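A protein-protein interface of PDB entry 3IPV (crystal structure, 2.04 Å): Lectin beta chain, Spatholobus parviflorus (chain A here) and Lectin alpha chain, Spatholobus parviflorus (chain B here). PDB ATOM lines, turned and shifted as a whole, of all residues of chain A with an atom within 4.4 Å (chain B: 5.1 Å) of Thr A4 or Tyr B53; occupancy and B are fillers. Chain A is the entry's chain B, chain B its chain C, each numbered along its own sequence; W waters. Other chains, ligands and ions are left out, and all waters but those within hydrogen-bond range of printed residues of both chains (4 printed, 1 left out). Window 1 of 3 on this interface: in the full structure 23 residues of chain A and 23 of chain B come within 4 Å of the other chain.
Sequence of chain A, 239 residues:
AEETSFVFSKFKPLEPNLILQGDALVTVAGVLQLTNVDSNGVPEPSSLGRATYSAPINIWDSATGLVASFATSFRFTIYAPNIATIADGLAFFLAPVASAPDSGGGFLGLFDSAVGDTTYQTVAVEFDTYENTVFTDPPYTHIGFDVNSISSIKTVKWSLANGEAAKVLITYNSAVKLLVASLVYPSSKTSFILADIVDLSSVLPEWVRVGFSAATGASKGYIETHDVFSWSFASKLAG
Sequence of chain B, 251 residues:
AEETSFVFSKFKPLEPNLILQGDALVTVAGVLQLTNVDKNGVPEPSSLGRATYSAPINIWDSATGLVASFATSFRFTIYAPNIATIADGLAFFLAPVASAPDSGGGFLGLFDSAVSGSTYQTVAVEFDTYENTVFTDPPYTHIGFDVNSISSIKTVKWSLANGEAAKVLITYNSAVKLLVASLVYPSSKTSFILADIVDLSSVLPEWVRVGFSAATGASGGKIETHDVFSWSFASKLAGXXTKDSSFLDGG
Of the 18 printed residues of chain B, 7 touch a printed residue of chain A. Hydrophobic or aromatic side chains of chain B within 4 Å of the printed part of chain A: Phe B6, Tyr B53 and Ala B55. Hydrophobic or aromatic side chains of chain A that line the printed part of chain B: Tyr A53 and Ala A55. Among the printed residues, 11 pairs touch across the chains.
The side-chain hydroxyl (OG) of Ser A5 lies within hydrogen-bond range of the side-chain hydroxyl (OG) of Ser B5. The backbone NH of Val B7 lies within hydrogen-bond range of the backbone carbonyl oxygen of Glu A3 (2.7 Å).
Among the printed residues, pairs that only touch across the chains: Glu A3 with Phe B6, Ala A55 with Ser B54, Tyr A53 with Ala B55, Ala A55 with Tyr B53, Tyr A53 with Thr B4, Thr A4 with Tyr B53, Ala A55 with Ala B55, Ser A5 with Thr B4 and Thr A4 with Ser B5.
O of Asn B17 lies within hydrogen-bond range of N of Ser B54 (2.9 Å). The backbone NH (N) of Tyr B53 is in hydrogen-bond range of the backbone carbonyl oxygen (O) of Val B210 (2.9 Å). O of Ser B54 sits at hydrogen-bond distance from NE of Arg B209 (3.2 Å). The backbone carbonyl oxygen of Thr A4 is in hydrogen-bond range of the backbone NH of Ser A235, 2.9 Å away.
Of the printed residues of chain B, Glu A3 touches Phe B6 (3.3 Å) and Val B7 (2.7 Å). Of chain B, only Ser B5 (3.8 Å) and Tyr B53 (3.7 Å) come within 4 Å of Thr A4. Printed residues of chain B within 4 Å of Ser A5: Thr B4 and Ser B5. Of the printed residues of chain B, Ala A55 touches Tyr B53, Ser B54 and Ala B55. Ile A57 touches none of the printed residues of chain B. Of the printed residues of chain A, Phe B6 touches Glu A3 (3.3 Å). Tyr B53 touches two residues of chain A. Printed residues of chain A within 4 Å of Ala B55: Tyr A53 (3.6 Å) and Ala A55 (3.7 Å).
Water W3 lies within hydrogen-bond range of the side-chain hydroxyl (OH) of Tyr A53 (2.6 Å), the side-chain hydroxyl (OH) of Tyr B53 (2.7 Å), the backbone carbonyl oxygen (O) of Ser A5 (3.2 Å) and the backbone carbonyl oxygen (O) of Ser B5 (3.3 Å). Water W1 bridges the side-chain hydroxyl (OH) of Tyr A53 (2.6 Å) and the side-chain hydroxyl (OG1) of Thr B4 (2.7 Å). Water W4 lies within hydrogen-bond range of the side-chain hydroxyl (OH) of Tyr B53 (2.8 Å), the side-chain hydroxyl (OG1) of Thr A4 (2.8 Å) and the side-chain amide nitrogen (ND2) of Asn B17 (3.0 Å). Water W2 lies within hydrogen-bond range of OG of Ser B5 (2.9 Å) and OG of Ser A5 (3.1 Å).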
ATOM      1  N   GLU A   3     -28.854  -4.731  28.948  1.00  0.00           N
ATOM      2  CA  GLU A   3     -28.782  -6.169  28.926  1.00  0.00           C
ATOM      3  C   GLU A   3     -28.574  -6.709  27.541  1.00  0.00           C
ATOM      4  O   GLU A   3     -29.052  -6.092  26.544  1.00  0.00           O
ATOM      5  CB  GLU A   3     -30.130  -6.763  29.417  1.00  0.00           C
ATOM      6  CG  GLU A   3     -30.522  -6.215  30.721  1.00  0.00           C
ATOM      7  CD  GLU A   3     -31.807  -6.811  31.175  1.00  0.00           C
ATOM      8  OE1 GLU A   3     -32.030  -7.978  30.828  1.00  0.00           O
ATOM      9  OE2 GLU A   3     -32.583  -6.133  31.865  1.00  0.00           O
ATOM     10  N   THR A   4     -27.902  -7.877  27.513  1.00  0.00           N
ATOM     11  CA  THR A   4     -27.656  -8.659  26.319  1.00  0.00           C
ATOM     12  C   THR A   4     -27.832 -10.123  26.594  1.00  0.00           C
ATOM     13  O   THR A   4     -27.285 -10.586  27.564  1.00  0.00           O
ATOM     14  CB  THR A   4     -26.182  -8.585  25.855  1.00  0.00           C
ATOM     15  OG1 THR A   4     -25.809  -7.229  25.550  1.00  0.00           O
ATOM     16  CG2 THR A   4     -26.027  -9.480  24.598  1.00  0.00           C
ATOM     17  N   SER A   5     -28.542 -10.857  25.705  1.00  0.00           N
ATOM     18  CA  SER A   5     -28.612 -12.271  25.836  1.00  0.00           C
ATOM     19  C   SER A   5     -28.827 -12.961  24.471  1.00  0.00           C
ATOM     20  O   SER A   5     -29.303 -12.349  23.472  1.00  0.00           O
ATOM     21  CB  SER A   5     -29.726 -12.724  26.842  1.00  0.00           C
ATOM     22  OG  SER A   5     -30.996 -12.524  26.301  1.00  0.00           O
ATOM     23  N   TYR A  53     -19.392 -14.481  20.368  1.00  0.00           N
ATOM     24  CA  TYR A  53     -20.588 -13.771  19.962  1.00  0.00           C
ATOM     25  C   TYR A  53     -20.284 -12.426  19.303  1.00  0.00           C
ATOM     26  O   TYR A  53     -19.469 -11.652  19.804  1.00  0.00           O
ATOM     27  CB  TYR A  53     -21.460 -13.512  21.176  1.00  0.00           C
ATOM     28  CG  TYR A  53     -22.850 -13.028  20.828  1.00  0.00           C
ATOM     29  CD1 TYR A  53     -23.687 -13.800  20.001  1.00  0.00           C
ATOM     30  CD2 TYR A  53     -23.301 -11.742  21.264  1.00  0.00           C
ATOM     31  CE1 TYR A  53     -25.012 -13.364  19.705  1.00  0.00           C
ATOM     32  CE2 TYR A  53     -24.568 -11.257  20.890  1.00  0.00           C
ATOM     33  CZ  TYR A  53     -25.449 -12.095  20.163  1.00  0.00           C
ATOM     34  OH  TYR A  53     -26.756 -11.661  19.835  1.00  0.00           O
ATOM     35  N   ALA A  55     -21.739  -9.373  18.900  1.00  0.00           N
ATOM     36  CA  ALA A  55     -21.974  -8.129  19.590  1.00  0.00           C
ATOM     37  C   ALA A  55     -21.193  -7.954  20.914  1.00  0.00           C
ATOM     38  O   ALA A  55     -21.073  -8.836  21.717  1.00  0.00           O
ATOM     39  CB  ALA A  55     -23.468  -7.877  19.780  1.00  0.00           C
ATOM     40  N   ILE A  57     -20.510  -6.809  24.707  1.00  0.00           N
ATOM     41  CA  ILE A  57     -21.312  -6.871  25.944  1.00  0.00           C
ATOM     42  C   ILE A  57     -20.791  -5.751  26.812  1.00  0.00           C
ATOM     43  O   ILE A  57     -19.582  -5.632  27.005  1.00  0.00           O
ATOM     44  CB  ILE A  57     -21.091  -8.222  26.751  1.00  0.00           C
ATOM     45  CG1 ILE A  57     -21.133  -9.504  25.852  1.00  0.00           C
ATOM     46  CG2 ILE A  57     -22.053  -8.334  27.932  1.00  0.00           C
ATOM     47  CD1 ILE A  57     -22.314  -9.595  25.023  1.00  0.00           C
ATOM     48  N   PHE A 233     -26.349 -17.241  27.046  1.00  0.00           N
ATOM     49  CA  PHE A 233     -25.657 -16.139  27.761  1.00  0.00           C
ATOM     50  C   PHE A 233     -26.624 -15.019  28.033  1.00  0.00           C
ATOM     51  O   PHE A 233     -27.483 -14.664  27.169  1.00  0.00           O
ATOM     52  CB  PHE A 233     -24.431 -15.568  26.953  1.00  0.00           C
ATOM     53  CG  PHE A 233     -23.687 -14.431  27.656  1.00  0.00           C
ATOM     54  CD1 PHE A 233     -24.087 -13.102  27.516  1.00  0.00           C
ATOM     55  CD2 PHE A 233     -22.552 -14.695  28.463  1.00  0.00           C
ATOM     56  CE1 PHE A 233     -23.417 -12.079  28.214  1.00  0.00           C
ATOM     57  CE2 PHE A 233     -21.883 -13.674  29.120  1.00  0.00           C
ATOM     58  CZ  PHE A 233     -22.316 -12.361  28.988  1.00  0.00           C
ATOM     59  N   ALA A 234     -26.455 -14.386  29.195  1.00  0.00           N
ATOM     60  CA  ALA A 234     -27.318 -13.271  29.570  1.00  0.00           C
ATOM     61  C   ALA A 234     -26.544 -12.384  30.574  1.00  0.00           C
ATOM     62  O   ALA A 234     -25.872 -12.901  31.480  1.00  0.00           O
ATOM     63  CB  ALA A 234     -28.665 -13.780  30.144  1.00  0.00           C
ATOM     64  N   SER A 235     -26.531 -11.074  30.326  1.00  0.00           N
ATOM     65  CA  SER A 235     -25.785 -10.170  31.182  1.00  0.00           C
ATOM     66  C   SER A 235     -26.800  -9.127  31.600  1.00  0.00           C
ATOM     67  O   SER A 235     -27.782  -8.840  30.853  1.00  0.00           O
ATOM     68  CB  SER A 235     -24.575  -9.564  30.463  1.00  0.00           C
ATOM     69  OG  SER A 235     -25.011  -8.662  29.409  1.00  0.00           O
ATOM     70  N   THR B   4     -32.294 -14.198  20.370  1.00  0.00           N
ATOM     71  CA  THR B   4     -31.467 -13.021  20.446  1.00  0.00           C
ATOM     72  C   THR B   4     -32.280 -11.983  21.141  1.00  0.00           C
ATOM     73  O   THR B   4     -33.410 -11.768  20.740  1.00  0.00           O
ATOM     74  CB  THR B   4     -31.149 -12.432  19.054  1.00  0.00           C
ATOM     75  OG1 THR B   4     -30.372 -13.360  18.315  1.00  0.00           O
ATOM     76  CG2 THR B   4     -30.263 -11.161  19.268  1.00  0.00           C
ATOM     77  N   SER B   5     -31.718 -11.356  22.173  1.00  0.00           N
ATOM     78  CA  SER B   5     -32.391 -10.258  22.838  1.00  0.00           C
ATOM     79  C   SER B   5     -31.449  -9.177  23.371  1.00  0.00           C
ATOM     80  O   SER B   5     -30.313  -9.433  23.711  1.00  0.00           O
ATOM     81  CB  SER B   5     -33.379 -10.765  23.958  1.00  0.00           C
ATOM     82  OG  SER B   5     -32.702 -11.366  25.044  1.00  0.00           O
ATOM     83  N   PHE B   6     -31.958  -7.952  23.517  1.00  0.00           N
ATOM     84  CA  PHE B   6     -31.190  -6.983  24.187  1.00  0.00           C
ATOM     85  C   PHE B   6     -32.078  -5.972  24.786  1.00  0.00           C
ATOM     86  O   PHE B   6     -33.230  -5.772  24.337  1.00  0.00           O
ATOM     87  CB  PHE B   6     -30.204  -6.300  23.198  1.00  0.00           C
ATOM     88  CG  PHE B   6     -30.816  -5.978  21.862  1.00  0.00           C
ATOM     89  CD1 PHE B   6     -30.847  -6.926  20.836  1.00  0.00           C
ATOM     90  CD2 PHE B   6     -31.399  -4.744  21.654  1.00  0.00           C
ATOM     91  CE1 PHE B   6     -31.406  -6.618  19.567  1.00  0.00           C
ATOM     92  CE2 PHE B   6     -31.954  -4.417  20.394  1.00  0.00           C
ATOM     93  CZ  PHE B   6     -31.950  -5.374  19.343  1.00  0.00           C
ATOM     94  N   VAL B   7     -31.531  -5.253  25.768  1.00  0.00           N
ATOM     95  CA  VAL B   7     -32.218  -4.044  26.267  1.00  0.00           C
ATOM     96  C   VAL B   7     -31.254  -2.835  26.403  1.00  0.00           C
ATOM     97  O   VAL B   7     -30.168  -2.941  27.028  1.00  0.00           O
ATOM     98  CB  VAL B   7     -32.941  -4.277  27.631  1.00  0.00           C
ATOM     99  CG1 VAL B   7     -33.583  -2.964  28.172  1.00  0.00           C
ATOM    100  CG2 VAL B   7     -33.930  -5.282  27.542  1.00  0.00           C
ATOM    101  N   PHE B   8     -31.669  -1.716  25.808  1.00  0.00           N
ATOM    102  CA  PHE B   8     -31.069  -0.402  26.003  1.00  0.00           C
ATOM    103  C   PHE B   8     -32.069   0.413  26.797  1.00  0.00           C
ATOM    104  O   PHE B   8     -33.035   0.962  26.206  1.00  0.00           O
ATOM    105  CB  PHE B   8     -30.842   0.328  24.656  1.00  0.00           C
ATOM    106  CG  PHE B   8     -29.902  -0.379  23.722  1.00  0.00           C
ATOM    107  CD1 PHE B   8     -30.371  -1.309  22.790  1.00  0.00           C
ATOM    108  CD2 PHE B   8     -28.561  -0.055  23.690  1.00  0.00           C
ATOM    109  CE1 PHE B   8     -29.538  -1.949  21.890  1.00  0.00           C
ATOM    110  CE2 PHE B   8     -27.687  -0.698  22.779  1.00  0.00           C
ATOM    111  CZ  PHE B   8     -28.206  -1.650  21.856  1.00  0.00           C
ATOM    112  N   ASN B  17     -22.277  -1.917  20.473  1.00  0.00           N
ATOM    113  CA  ASN B  17     -23.331  -2.856  20.018  1.00  0.00           C
ATOM    114  C   ASN B  17     -24.480  -2.185  19.220  1.00  0.00           C
ATOM    115  O   ASN B  17     -25.486  -2.838  18.920  1.00  0.00           O
ATOM    116  CB  ASN B  17     -23.900  -3.639  21.213  1.00  0.00           C
ATOM    117  CG  ASN B  17     -24.503  -2.734  22.296  1.00  0.00           C
ATOM    118  OD1 ASN B  17     -24.385  -1.481  22.244  1.00  0.00           O
ATOM    119  ND2 ASN B  17     -25.161  -3.366  23.305  1.00  0.00           N
ATOM    120  N   LEU B  18     -24.354  -0.880  18.931  1.00  0.00           N
ATOM    121  CA  LEU B  18     -25.228  -0.217  17.978  1.00  0.00           C
ATOM    122  C   LEU B  18     -24.401   0.163  16.713  1.00  0.00           C
ATOM    123  O   LEU B  18     -23.227   0.586  16.809  1.00  0.00           O
ATOM    124  CB  LEU B  18     -25.785   1.074  18.548  1.00  0.00           C
ATOM    125  CG  LEU B  18     -27.196   1.301  19.087  1.00  0.00           C
ATOM    126  CD1 LEU B  18     -27.485   2.820  19.333  1.00  0.00           C
ATOM    127  CD2 LEU B  18     -28.225   0.692  18.192  1.00  0.00           C
ATOM    128  N   ILE B  19     -25.005   0.078  15.545  1.00  0.00           N
ATOM    129  CA  ILE B  19     -24.372   0.636  14.357  1.00  0.00           C
ATOM    130  C   ILE B  19     -25.149   1.885  13.944  1.00  0.00           C
ATOM    131  O   ILE B  19     -26.333   1.807  13.512  1.00  0.00           O
ATOM    132  CB  ILE B  19     -24.311  -0.352  13.174  1.00  0.00           C
ATOM    133  CG1 ILE B  19     -23.584  -1.641  13.576  1.00  0.00           C
ATOM    134  CG2 ILE B  19     -23.577   0.267  11.978  1.00  0.00           C
ATOM    135  CD1 ILE B  19     -23.897  -2.797  12.625  1.00  0.00           C
ATOM    136  N   ALA B  51     -30.001   3.562  13.144  1.00  0.00           N
ATOM    137  CA  ALA B  51     -29.269   2.856  14.178  1.00  0.00           C
ATOM    138  C   ALA B  51     -29.793   1.427  14.175  1.00  0.00           C
ATOM    139  O   ALA B  51     -30.993   1.214  14.192  1.00  0.00           O
ATOM    140  CB  ALA B  51     -29.533   3.497  15.482  1.00  0.00           C
ATOM    141  N   THR B  52     -28.911   0.465  14.199  1.00  0.00           N
ATOM    142  CA  THR B  52     -29.316  -0.936  14.131  1.00  0.00           C
ATOM    143  C   THR B  52     -28.457  -1.748  15.083  1.00  0.00           C
ATOM    144  O   THR B  52     -27.269  -1.441  15.301  1.00  0.00           O
ATOM    145  CB  THR B  52     -29.148  -1.561  12.731  1.00  0.00           C
ATOM    146  OG1 THR B  52     -27.814  -1.307  12.274  1.00  0.00           O
ATOM    147  CG2 THR B  52     -30.171  -1.026  11.743  1.00  0.00           C
ATOM    148  N   TYR B  53     -29.077  -2.764  15.708  1.00  0.00           N
ATOM    149  CA  TYR B  53     -28.314  -3.615  16.656  1.00  0.00           C
ATOM    150  C   TYR B  53     -27.200  -4.326  15.928  1.00  0.00           C
ATOM    151  O   TYR B  53     -27.365  -4.781  14.804  1.00  0.00           O
ATOM    152  CB  TYR B  53     -29.213  -4.628  17.365  1.00  0.00           C
ATOM    153  CG  TYR B  53     -28.514  -5.456  18.440  1.00  0.00           C
ATOM    154  CD1 TYR B  53     -27.977  -4.845  19.604  1.00  0.00           C
ATOM    155  CD2 TYR B  53     -28.413  -6.839  18.318  1.00  0.00           C
ATOM    156  CE1 TYR B  53     -27.364  -5.602  20.581  1.00  0.00           C
ATOM    157  CE2 TYR B  53     -27.758  -7.626  19.281  1.00  0.00           C
ATOM    158  CZ  TYR B  53     -27.279  -6.995  20.426  1.00  0.00           C
ATOM    159  OH  TYR B  53     -26.663  -7.757  21.399  1.00  0.00           O
ATOM    160  N   SER B  54     -26.080  -4.493  16.600  1.00  0.00           N
ATOM    161  CA  SER B  54     -24.904  -4.858  15.915  1.00  0.00           C
ATOM    162  C   SER B  54     -24.863  -6.343  15.521  1.00  0.00           C
ATOM    163  O   SER B  54     -24.234  -6.666  14.504  1.00  0.00           O
ATOM    164  CB  SER B  54     -23.630  -4.376  16.644  1.00  0.00           C
ATOM    165  OG  SER B  54     -23.045  -5.393  17.430  1.00  0.00           O
ATOM    166  N   ALA B  55     -25.601  -7.195  16.258  1.00  0.00           N
ATOM    167  CA  ALA B  55     -25.678  -8.612  15.930  1.00  0.00           C
ATOM    168  C   ALA B  55     -26.833  -9.007  14.947  1.00  0.00           C
ATOM    169  O   ALA B  55     -27.950  -8.550  15.075  1.00  0.00           O
ATOM    170  CB  ALA B  55     -25.684  -9.473  17.215  1.00  0.00           C
ATOM    171  N   ILE B  57     -29.743 -11.148  13.423  1.00  0.00           N
ATOM    172  CA  ILE B  57     -30.788 -11.941  14.027  1.00  0.00           C
ATOM    173  C   ILE B  57     -31.314 -13.037  13.044  1.00  0.00           C
ATOM    174  O   ILE B  57     -31.609 -12.732  11.897  1.00  0.00           O
ATOM    175  CB  ILE B  57     -31.885 -10.972  14.441  1.00  0.00           C
ATOM    176  CG1 ILE B  57     -31.247 -10.042  15.547  1.00  0.00           C
ATOM    177  CG2 ILE B  57     -33.144 -11.712  14.914  1.00  0.00           C
ATOM    178  CD1 ILE B  57     -31.984  -8.900  15.907  1.00  0.00           C
ATOM    179  N   ARG B 209     -30.650  -7.515  10.196  1.00  0.00           N
ATOM    180  CA  ARG B 209     -30.375  -6.627  11.342  1.00  0.00           C
ATOM    181  C   ARG B 209     -31.605  -5.838  11.551  1.00  0.00           C
ATOM    182  O   ARG B 209     -32.415  -5.661  10.594  1.00  0.00           O
ATOM    183  CB  ARG B 209     -29.201  -5.689  11.082  1.00  0.00           C
ATOM    184  CG  ARG B 209     -27.832  -6.351  11.399  1.00  0.00           C
ATOM    185  CD  ARG B 209     -26.625  -5.376  11.046  1.00  0.00           C
ATOM    186  NE  ARG B 209     -25.347  -5.800  11.629  1.00  0.00           N
ATOM    187  CZ  ARG B 209     -24.269  -6.058  10.894  1.00  0.00           C
ATOM    188  NH1 ARG B 209     -24.345  -5.941   9.579  1.00  0.00           N
ATOM    189  NH2 ARG B 209     -23.114  -6.423  11.458  1.00  0.00           N
ATOM    190  N   VAL B 210     -31.769  -5.322  12.761  1.00  0.00           N
ATOM    191  CA  VAL B 210     -32.985  -4.618  13.047  1.00  0.00           C
ATOM    192  C   VAL B 210     -32.627  -3.287  13.663  1.00  0.00           C
ATOM    193  O   VAL B 210     -31.573  -3.166  14.226  1.00  0.00           O
ATOM    194  CB  VAL B 210     -33.915  -5.419  14.033  1.00  0.00           C
ATOM    195  CG1 VAL B 210     -34.314  -6.832  13.467  1.00  0.00           C
ATOM    196  CG2 VAL B 210     -33.303  -5.545  15.382  1.00  0.00           C
ATOM    197  N   GLY B 211     -33.513  -2.307  13.564  1.00  0.00           N
ATOM    198  CA  GLY B 211     -33.270  -1.008  14.162  1.00  0.00           C
ATOM    199  C   GLY B 211     -34.278   0.027  13.747  1.00  0.00           C
ATOM    200  O   GLY B 211     -35.425  -0.303  13.465  1.00  0.00           O
ATOM    201  N   TRP B 231     -34.984   1.038  24.119  1.00  0.00           N
ATOM    202  CA  TRP B 231     -35.313   0.058  23.083  1.00  0.00           C
ATOM    203  C   TRP B 231     -34.968  -1.326  23.676  1.00  0.00           C
ATOM    204  O   TRP B 231     -33.814  -1.585  24.150  1.00  0.00           O
ATOM    205  CB  TRP B 231     -34.478   0.305  21.806  1.00  0.00           C
ATOM    206  CG  TRP B 231     -34.696  -0.775  20.640  1.00  0.00           C
ATOM    207  CD1 TRP B 231     -35.856  -1.473  20.342  1.00  0.00           C
ATOM    208  CD2 TRP B 231     -33.746  -1.129  19.646  1.00  0.00           C
ATOM    209  NE1 TRP B 231     -35.656  -2.258  19.226  1.00  0.00           N
ATOM    210  CE2 TRP B 231     -34.351  -2.078  18.799  1.00  0.00           C
ATOM    211  CE3 TRP B 231     -32.408  -0.737  19.390  1.00  0.00           C
ATOM    212  CZ2 TRP B 231     -33.673  -2.633  17.728  1.00  0.00           C
ATOM    213  CZ3 TRP B 231     -31.744  -1.274  18.314  1.00  0.00           C
ATOM    214  CH2 TRP B 231     -32.369  -2.232  17.495  1.00  0.00           C
HETATM  215  O   HOH W   1     -27.817 -12.630  17.617  1.00  0.00           O
HETATM  216  O   HOH W   2     -32.429 -14.116  24.034  1.00  0.00           O
HETATM  217  O   HOH W   3     -27.875 -10.164  21.585  1.00  0.00           O
HETATM  218  O   HOH W   4     -24.837  -6.353  23.036  1.00  0.00           O
